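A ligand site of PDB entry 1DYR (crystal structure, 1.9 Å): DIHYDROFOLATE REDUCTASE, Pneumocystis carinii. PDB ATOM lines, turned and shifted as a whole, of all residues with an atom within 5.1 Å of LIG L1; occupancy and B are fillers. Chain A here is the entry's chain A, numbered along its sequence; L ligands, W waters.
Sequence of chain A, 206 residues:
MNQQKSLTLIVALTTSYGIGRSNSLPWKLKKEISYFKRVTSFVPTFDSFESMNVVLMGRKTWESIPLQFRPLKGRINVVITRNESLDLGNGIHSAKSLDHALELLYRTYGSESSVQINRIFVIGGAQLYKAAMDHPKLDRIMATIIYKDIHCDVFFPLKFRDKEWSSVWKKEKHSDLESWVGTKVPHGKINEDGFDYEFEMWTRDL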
ATOM      1  N   ILE A  10     -21.590   3.232  19.981  1.00  0.00           N
ATOM      2  CA  ILE A  10     -20.296   3.362  19.323  1.00  0.00           C
ATOM      3  C   ILE A  10     -20.445   3.220  17.816  1.00  0.00           C
ATOM      4  O   ILE A  10     -21.090   2.277  17.370  1.00  0.00           O
ATOM      5  CB  ILE A  10     -19.285   2.355  20.002  1.00  0.00           C
ATOM      6  CG1 ILE A  10     -17.891   2.549  19.314  1.00  0.00           C
ATOM      7  CG2 ILE A  10     -19.786   0.878  19.869  1.00  0.00           C
ATOM      8  CD1 ILE A  10     -16.670   2.241  20.184  1.00  0.00           C
ATOM      9  N   VAL A  11     -19.839   4.186  17.080  1.00  0.00           N
ATOM     10  CA  VAL A  11     -20.032   4.320  15.627  1.00  0.00           C
ATOM     11  C   VAL A  11     -18.822   4.946  14.970  1.00  0.00           C
ATOM     12  O   VAL A  11     -18.142   5.703  15.672  1.00  0.00           O
ATOM     13  CB  VAL A  11     -21.308   5.201  15.366  1.00  0.00           C
ATOM     14  CG1 VAL A  11     -21.214   6.523  16.033  1.00  0.00           C
ATOM     15  CG2 VAL A  11     -21.676   5.273  13.910  1.00  0.00           C
ATOM     16  N   ALA A  12     -18.555   4.591  13.747  1.00  0.00           N
ATOM     17  CA  ALA A  12     -17.527   5.220  12.896  1.00  0.00           C
ATOM     18  C   ALA A  12     -18.288   5.810  11.700  1.00  0.00           C
ATOM     19  O   ALA A  12     -19.043   5.043  11.105  1.00  0.00           O
ATOM     20  CB  ALA A  12     -16.421   4.261  12.381  1.00  0.00           C
ATOM     21  N   SER A  24     -21.380  -3.686   4.353  1.00  0.00           N
ATOM     22  CA  SER A  24     -19.996  -3.686   4.856  1.00  0.00           C
ATOM     23  C   SER A  24     -19.587  -2.257   5.187  1.00  0.00           C
ATOM     24  O   SER A  24     -20.275  -1.291   4.828  1.00  0.00           O
ATOM     25  CB  SER A  24     -19.011  -4.172   3.774  1.00  0.00           C
ATOM     26  OG  SER A  24     -19.551  -5.212   3.002  1.00  0.00           O
ATOM     27  N   LEU A  25     -18.443  -2.133   5.810  1.00  0.00           N
ATOM     28  CA  LEU A  25     -17.727  -0.835   5.921  1.00  0.00           C
ATOM     29  C   LEU A  25     -17.018  -0.525   4.616  1.00  0.00           C
ATOM     30  O   LEU A  25     -16.291  -1.369   4.033  1.00  0.00           O
ATOM     31  CB  LEU A  25     -16.831  -1.024   7.140  1.00  0.00           C
ATOM     32  CG  LEU A  25     -17.151  -0.575   8.526  1.00  0.00           C
ATOM     33  CD1 LEU A  25     -18.583  -0.389   8.902  1.00  0.00           C
ATOM     34  CD2 LEU A  25     -16.453  -1.561   9.488  1.00  0.00           C
ATOM     35  N   GLU A  32      -8.610   1.378  13.796  1.00  0.00           N
ATOM     36  CA  GLU A  32      -9.993   1.766  14.184  1.00  0.00           C
ATOM     37  C   GLU A  32     -10.627   0.558  14.853  1.00  0.00           C
ATOM     38  O   GLU A  32     -11.225   0.712  15.942  1.00  0.00           O
ATOM     39  CB  GLU A  32     -10.799   2.379  13.092  1.00  0.00           C
ATOM     40  CG  GLU A  32     -12.065   3.176  13.355  1.00  0.00           C
ATOM     41  CD  GLU A  32     -13.183   2.581  14.183  1.00  0.00           C
ATOM     42  OE1 GLU A  32     -13.598   1.475  13.768  1.00  0.00           O
ATOM     43  OE2 GLU A  32     -13.611   3.146  15.176  1.00  0.00           O
ATOM     44  N   ILE A  33     -10.413  -0.622  14.292  1.00  0.00           N
ATOM     45  CA  ILE A  33     -10.981  -1.865  14.876  1.00  0.00           C
ATOM     46  C   ILE A  33     -10.319  -2.186  16.204  1.00  0.00           C
ATOM     47  O   ILE A  33     -11.033  -2.646  17.120  1.00  0.00           O
ATOM     48  CB  ILE A  33     -11.083  -3.059  13.887  1.00  0.00           C
ATOM     49  CG1 ILE A  33     -11.952  -2.849  12.631  1.00  0.00           C
ATOM     50  CG2 ILE A  33     -11.403  -4.416  14.590  1.00  0.00           C
ATOM     51  CD1 ILE A  33     -13.442  -2.548  12.808  1.00  0.00           C
ATOM     52  N   PHE A  36     -11.959  -0.051  18.667  1.00  0.00           N
ATOM     53  CA  PHE A  36     -13.325  -0.616  18.922  1.00  0.00           C
ATOM     54  C   PHE A  36     -13.236  -1.685  19.996  1.00  0.00           C
ATOM     55  O   PHE A  36     -13.958  -1.707  21.009  1.00  0.00           O
ATOM     56  CB  PHE A  36     -14.031  -0.997  17.641  1.00  0.00           C
ATOM     57  CG  PHE A  36     -15.266  -1.836  17.841  1.00  0.00           C
ATOM     58  CD1 PHE A  36     -16.488  -1.240  18.096  1.00  0.00           C
ATOM     59  CD2 PHE A  36     -15.181  -3.208  17.862  1.00  0.00           C
ATOM     60  CE1 PHE A  36     -17.630  -2.019  18.276  1.00  0.00           C
ATOM     61  CE2 PHE A  36     -16.278  -4.033  18.112  1.00  0.00           C
ATOM     62  CZ  PHE A  36     -17.523  -3.397  18.302  1.00  0.00           C
ATOM     63  N   THR A  61     -26.010  -6.565  10.995  1.00  0.00           N
ATOM     64  CA  THR A  61     -24.627  -6.349  11.497  1.00  0.00           C
ATOM     65  C   THR A  61     -24.035  -7.673  11.923  1.00  0.00           C
ATOM     66  O   THR A  61     -22.864  -7.959  11.540  1.00  0.00           O
ATOM     67  CB  THR A  61     -24.584  -5.281  12.660  1.00  0.00           C
ATOM     68  OG1 THR A  61     -25.064  -4.053  12.003  1.00  0.00           O
ATOM     69  CG2 THR A  61     -23.196  -5.051  13.263  1.00  0.00           C
ATOM     70  N   SER A  64     -22.902  -9.342   9.098  1.00  0.00           N
ATOM     71  CA  SER A  64     -21.779  -8.663   8.435  1.00  0.00           C
ATOM     72  C   SER A  64     -20.430  -8.977   9.029  1.00  0.00           C
ATOM     73  O   SER A  64     -19.435  -8.811   8.297  1.00  0.00           O
ATOM     74  CB  SER A  64     -22.000  -7.160   8.328  1.00  0.00           C
ATOM     75  OG  SER A  64     -23.190  -7.000   7.515  1.00  0.00           O
ATOM     76  N   ILE A  65     -20.364  -9.364  10.293  1.00  0.00           N
ATOM     77  CA  ILE A  65     -19.067  -9.581  10.942  1.00  0.00           C
ATOM     78  C   ILE A  65     -18.410 -10.839  10.397  1.00  0.00           C
ATOM     79  O   ILE A  65     -19.005 -11.931  10.407  1.00  0.00           O
ATOM     80  CB  ILE A  65     -19.172  -9.452  12.498  1.00  0.00           C
ATOM     81  CG1 ILE A  65     -19.453  -7.939  12.799  1.00  0.00           C
ATOM     82  CG2 ILE A  65     -17.885  -9.945  13.244  1.00  0.00           C
ATOM     83  CD1 ILE A  65     -19.954  -7.574  14.204  1.00  0.00           C
ATOM     84  N   PRO A  66     -17.180 -10.642   9.912  1.00  0.00           N
ATOM     85  CA  PRO A  66     -16.353 -11.764   9.443  1.00  0.00           C
ATOM     86  C   PRO A  66     -16.511 -12.935  10.398  1.00  0.00           C
ATOM     87  O   PRO A  66     -16.305 -12.793  11.609  1.00  0.00           O
ATOM     88  CB  PRO A  66     -14.921 -11.199   9.428  1.00  0.00           C
ATOM     89  CG  PRO A  66     -15.138  -9.711   9.226  1.00  0.00           C
ATOM     90  CD  PRO A  66     -16.380  -9.407  10.087  1.00  0.00           C
ATOM     91  N   PHE A  69     -14.599 -13.475  13.384  1.00  0.00           N
ATOM     92  CA  PHE A  69     -14.646 -12.431  14.426  1.00  0.00           C
ATOM     93  C   PHE A  69     -15.855 -12.617  15.343  1.00  0.00           C
ATOM     94  O   PHE A  69     -16.072 -11.917  16.332  1.00  0.00           O
ATOM     95  CB  PHE A  69     -14.687 -11.076  13.698  1.00  0.00           C
ATOM     96  CG  PHE A  69     -13.387 -10.517  13.220  1.00  0.00           C
ATOM     97  CD1 PHE A  69     -12.490 -11.280  12.454  1.00  0.00           C
ATOM     98  CD2 PHE A  69     -13.076  -9.173  13.502  1.00  0.00           C
ATOM     99  CE1 PHE A  69     -11.277 -10.752  12.045  1.00  0.00           C
ATOM    100  CE2 PHE A  69     -11.841  -8.630  13.152  1.00  0.00           C
ATOM    101  CZ  PHE A  69     -10.961  -9.433  12.387  1.00  0.00           C
ATOM    102  N   LEU A  72     -18.129 -11.876  19.227  1.00  0.00           N
ATOM    103  CA  LEU A  72     -17.161 -10.936  19.769  1.00  0.00           C
ATOM    104  C   LEU A  72     -16.628 -11.408  21.083  1.00  0.00           C
ATOM    105  O   LEU A  72     -17.279 -11.370  22.143  1.00  0.00           O
ATOM    106  CB  LEU A  72     -17.686  -9.506  19.651  1.00  0.00           C
ATOM    107  CG  LEU A  72     -18.082  -9.012  18.263  1.00  0.00           C
ATOM    108  CD1 LEU A  72     -18.785  -7.632  18.344  1.00  0.00           C
ATOM    109  CD2 LEU A  72     -16.874  -8.889  17.357  1.00  0.00           C
ATOM    110  N   ILE A 123     -23.803  -1.391  19.045  1.00  0.00           N
ATOM    111  CA  ILE A 123     -22.731  -1.300  18.047  1.00  0.00           C
ATOM    112  C   ILE A 123     -23.202  -1.265  16.629  1.00  0.00           C
ATOM    113  O   ILE A 123     -22.411  -1.407  15.668  1.00  0.00           O
ATOM    114  CB  ILE A 123     -21.677  -2.393  18.367  1.00  0.00           C
ATOM    115  CG1 ILE A 123     -22.291  -3.761  17.937  1.00  0.00           C
ATOM    116  CG2 ILE A 123     -21.195  -2.457  19.837  1.00  0.00           C
ATOM    117  CD1 ILE A 123     -21.342  -4.806  17.284  1.00  0.00           C
ATOM    118  N   GLY A 124     -24.546  -1.138  16.406  1.00  0.00           N
ATOM    119  CA  GLY A 124     -25.056  -0.928  15.054  1.00  0.00           C
ATOM    120  C   GLY A 124     -26.123  -1.927  14.647  1.00  0.00           C
ATOM    121  O   GLY A 124     -26.441  -2.793  15.475  1.00  0.00           O
ATOM    122  N   TYR A 129     -29.547   1.749  15.634  1.00  0.00           N
ATOM    123  CA  TYR A 129     -29.119   3.091  16.084  1.00  0.00           C
ATOM    124  C   TYR A 129     -30.347   4.005  16.219  1.00  0.00           C
ATOM    125  O   TYR A 129     -30.290   4.862  17.082  1.00  0.00           O
ATOM    126  CB  TYR A 129     -28.121   3.750  15.103  1.00  0.00           C
ATOM    127  CG  TYR A 129     -26.694   3.227  15.144  1.00  0.00           C
ATOM    128  CD1 TYR A 129     -26.056   2.871  16.359  1.00  0.00           C
ATOM    129  CD2 TYR A 129     -25.980   3.156  13.970  1.00  0.00           C
ATOM    130  CE1 TYR A 129     -24.736   2.403  16.352  1.00  0.00           C
ATOM    131  CE2 TYR A 129     -24.634   2.749  13.969  1.00  0.00           C
ATOM    132  CZ  TYR A 129     -24.042   2.407  15.147  1.00  0.00           C
ATOM    133  OH  TYR A 129     -22.712   1.961  15.146  1.00  0.00           O
ATOM    134  N   THR A 144     -16.050   7.742  15.878  1.00  0.00           N
ATOM    135  CA  THR A 144     -14.803   7.903  15.080  1.00  0.00           C
ATOM    136  C   THR A 144     -15.190   8.736  13.873  1.00  0.00           C
ATOM    137  O   THR A 144     -16.014   8.242  13.066  1.00  0.00           O
ATOM    138  CB  THR A 144     -14.193   6.472  14.719  1.00  0.00           C
ATOM    139  OG1 THR A 144     -13.963   5.767  15.961  1.00  0.00           O
ATOM    140  CG2 THR A 144     -12.918   6.564  13.887  1.00  0.00           C
HETATM  141  C1  LIG L   1     -16.752  -0.611  14.393  1.00  0.00           C
HETATM  142  N1  LIG L   1     -16.072   0.480  14.756  1.00  0.00           N
HETATM  143  C2  LIG L   1     -16.712   1.349  15.483  1.00  0.00           C
HETATM  144  N2  LIG L   1     -16.065   2.467  15.915  1.00  0.00           N
HETATM  145  N3  LIG L   1     -17.981   1.285  15.955  1.00  0.00           N
HETATM  146  C3  LIG L   1     -18.638   0.170  15.609  1.00  0.00           C
HETATM  147  N4  LIG L   1     -19.902  -0.019  16.055  1.00  0.00           N
HETATM  148  C4  LIG L   1     -18.027  -0.813  14.853  1.00  0.00           C
HETATM  149  C5  LIG L   1     -18.808  -2.079  14.469  1.00  0.00           C
HETATM  150  C6  LIG L   1     -18.140  -3.110  13.553  1.00  0.00           C
HETATM  151  C7  LIG L   1     -18.688  -3.271  12.287  1.00  0.00           C
HETATM  152  C8  LIG L   1     -18.152  -4.221  11.398  1.00  0.00           C
HETATM  153  O1  LIG L   1     -18.635  -4.374  10.128  1.00  0.00           O
HETATM  154  C9  LIG L   1     -19.912  -3.852   9.850  1.00  0.00           C
HETATM  155  C10 LIG L   1     -17.054  -4.994  11.827  1.00  0.00           C
HETATM  156  O2  LIG L   1     -16.488  -5.961  10.981  1.00  0.00           O
HETATM  157  C11 LIG L   1     -15.104  -5.822  11.079  1.00  0.00           C
HETATM  158  C12 LIG L   1     -16.529  -4.854  13.105  1.00  0.00           C
HETATM  159  O3  LIG L   1     -15.451  -5.688  13.412  1.00  0.00           O
HETATM  160  C13 LIG L   1     -15.231  -5.711  14.826  1.00  0.00           C
HETATM  161  C14 LIG L   1     -17.060  -3.914  14.003  1.00  0.00           C
HETATM  162  P1  LG2 L   2     -29.057  -3.657  11.441  1.00  0.00           P
HETATM  163  O1  LG2 L   2     -29.529  -2.703  12.433  1.00  0.00           O
HETATM  164  O2  LG2 L   2     -27.696  -4.176  11.810  1.00  0.00           O
HETATM  165  O3  LG2 L   2     -30.019  -4.922  11.355  1.00  0.00           O
HETATM  166  C1  LG2 L   2     -31.400  -4.684  10.974  1.00  0.00           C
HETATM  167  C2  LG2 L   2     -32.227  -5.832  11.525  1.00  0.00           C
HETATM  168  O4  LG2 L   2     -32.061  -5.932  12.953  1.00  0.00           O
HETATM  169  C3  LG2 L   2     -33.758  -5.716  11.272  1.00  0.00           C
HETATM  170  O5  LG2 L   2     -33.978  -6.054   9.893  1.00  0.00           O
HETATM  171  C4  LG2 L   2     -34.261  -6.623  12.434  1.00  0.00           C
HETATM  172  O6  LG2 L   2     -34.012  -8.061  12.385  1.00  0.00           O
HETATM  173  C5  LG2 L   2     -33.311  -6.107  13.505  1.00  0.00           C
HETATM  174  N1  LG2 L   2     -33.635  -4.917  14.193  1.00  0.00           N
HETATM  175  C6  LG2 L   2     -32.907  -3.715  14.184  1.00  0.00           C
HETATM  176  N2  LG2 L   2     -33.464  -2.781  14.924  1.00  0.00           N
HETATM  177  C7  LG2 L   2     -34.561  -3.413  15.468  1.00  0.00           C
HETATM  178  C8  LG2 L   2     -35.498  -2.972  16.420  1.00  0.00           C
HETATM  179  N3  LG2 L   2     -35.441  -1.740  16.933  1.00  0.00           N
HETATM  180  N4  LG2 L   2     -36.474  -3.826  16.738  1.00  0.00           N
HETATM  181  C9  LG2 L   2     -36.480  -5.075  16.201  1.00  0.00           C
HETATM  182  N5  LG2 L   2     -35.647  -5.602  15.369  1.00  0.00           N
HETATM  183  C10 LG2 L   2     -34.683  -4.696  15.025  1.00  0.00           C
HETATM  184  O7  LG2 L   2     -29.086  -3.160   9.999  1.00  0.00           O
HETATM  185  P2  LG2 L   2     -28.971  -1.964   8.949  1.00  0.00           P
HETATM  186  O8  LG2 L   2     -29.820  -0.842   9.310  1.00  0.00           O
HETATM  187  O9  LG2 L   2     -29.361  -2.505   7.644  1.00  0.00           O
HETATM  188  O10 LG2 L   2     -27.429  -1.554   9.018  1.00  0.00           O
HETATM  189  C11 LG2 L   2     -26.451  -2.409   8.386  1.00  0.00           C
HETATM  190  C12 LG2 L   2     -25.339  -1.564   7.852  1.00  0.00           C
HETATM  191  O11 LG2 L   2     -24.745  -0.781   8.950  1.00  0.00           O
HETATM  192  C13 LG2 L   2     -24.190  -2.310   7.166  1.00  0.00           C
HETATM  193  O12 LG2 L   2     -23.793  -1.568   5.973  1.00  0.00           O
HETATM  194  C14 LG2 L   2     -23.118  -2.275   8.251  1.00  0.00           C
HETATM  195  O13 LG2 L   2     -21.793  -2.429   7.682  1.00  0.00           O
HETATM  196  C15 LG2 L   2     -23.303  -0.900   8.817  1.00  0.00           C
HETATM  197  N6  LG2 L   2     -22.679  -0.688  10.139  1.00  0.00           N
HETATM  198  C16 LG2 L   2     -21.798   0.356  10.310  1.00  0.00           C
HETATM  199  C17 LG2 L   2     -21.228   0.590  11.518  1.00  0.00           C
HETATM  200  C18 LG2 L   2     -20.219   1.790  11.685  1.00  0.00           C
HETATM  201  O14 LG2 L   2     -19.787   1.983  12.806  1.00  0.00           O
HETATM  202  N7  LG2 L   2     -19.952   2.472  10.567  1.00  0.00           N
HETATM  203  C19 LG2 L   2     -21.492  -0.166  12.657  1.00  0.00           C
HETATM  204  C20 LG2 L   2     -22.404  -1.208  12.372  1.00  0.00           C
HETATM  205  C21 LG2 L   2     -23.017  -1.512  11.234  1.00  0.00           C
HETATM  206  P3  LG2 L   2     -35.018  -9.111  11.582  1.00  0.00           P
HETATM  207  O15 LG2 L   2     -35.227  -8.395  10.239  1.00  0.00           O
HETATM  208  O16 LG2 L   2     -34.318 -10.384  11.539  1.00  0.00           O
HETATM  209  O17 LG2 L   2     -36.239  -9.131  12.416  1.00  0.00           O
HETATM  210  O   HOH W   1     -17.906  -5.538   7.578  1.00  0.00           O
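Val 11 touches LIG L1. N of Ala 12 touches N2 of LIG L1, 3.9 Å away. CD2 of Leu 25 touches O1 of LIG L1, 3.6 Å away. CD1 of Ile 33 touches O3 of LIG L1 (3.8 Å). Phe 36 touches LIG L1 (CD1 to C3, 3.6 Å). CG1 of Ile 65 touches C10 of LIG L1, at 3.9 Å. CD of Pro 66 touches O2 of LIG L1, 3.6 Å away. Tyr 129 touches LIG L1. Thr 144 touches LIG L1. Within 4 Å of LIG L1: Ile 10, Val 11, Ala 12, Leu 25, Glu 32, Ile 33, Phe 36, Ile 65, Pro 66, Ile 123, Tyr 129 and Thr 144. Along chain A the residues within 4 Å of LIG L1 span positions 10 to 144.
The side-chain carboxylate (OE2) of Glu 32 sits at hydrogen-bond distance from a nitrogen (N2) of LIG L1. A nitrogen (N4) of LIG L1 lies within hydrogen-bond range of the backbone carbonyl oxygen (O) of Ile 123. N4 of LIG L1 sits at hydrogen-bond distance from O of Ile 10 (2.9 Å). The backbone NH (N) of Ala 12 sits at hydrogen-bond distance from an oxygen (O14) of LG2 L2, 3.0 Å away. The backbone carbonyl oxygen (O) of Ala 12 sits at hydrogen-bond distance from a nitrogen (N7) of LG2 L2 (2.8 Å). The backbone NH (N) of Thr 61 lies within hydrogen-bond range of an oxygen (O2) of LG2 L2. The side-chain hydroxyl (OG1) of Thr 61 lies within hydrogen-bond range of an oxygen (O2) of LG2 L2 (2.6 Å). O of Ser 24 lies close to O13 of LG2 L2 (3.4 Å).
The side-chain hydroxyl (OG1) of Thr 144 sits at hydrogen-bond distance from the side-chain carboxylate (OE2) of Glu 32 (2.8 Å). O of Ile 123 lies within hydrogen-bond range of OH of Tyr 129. The side-chain hydroxyl (OH) of Tyr 129 sits at hydrogen-bond distance from the backbone carbonyl oxygen (O) of Ile 10. The backbone carbonyl oxygen (O) of Val 11 lies within hydrogen-bond range of the backbone NH (N) of Thr 144 (2.9 Å).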
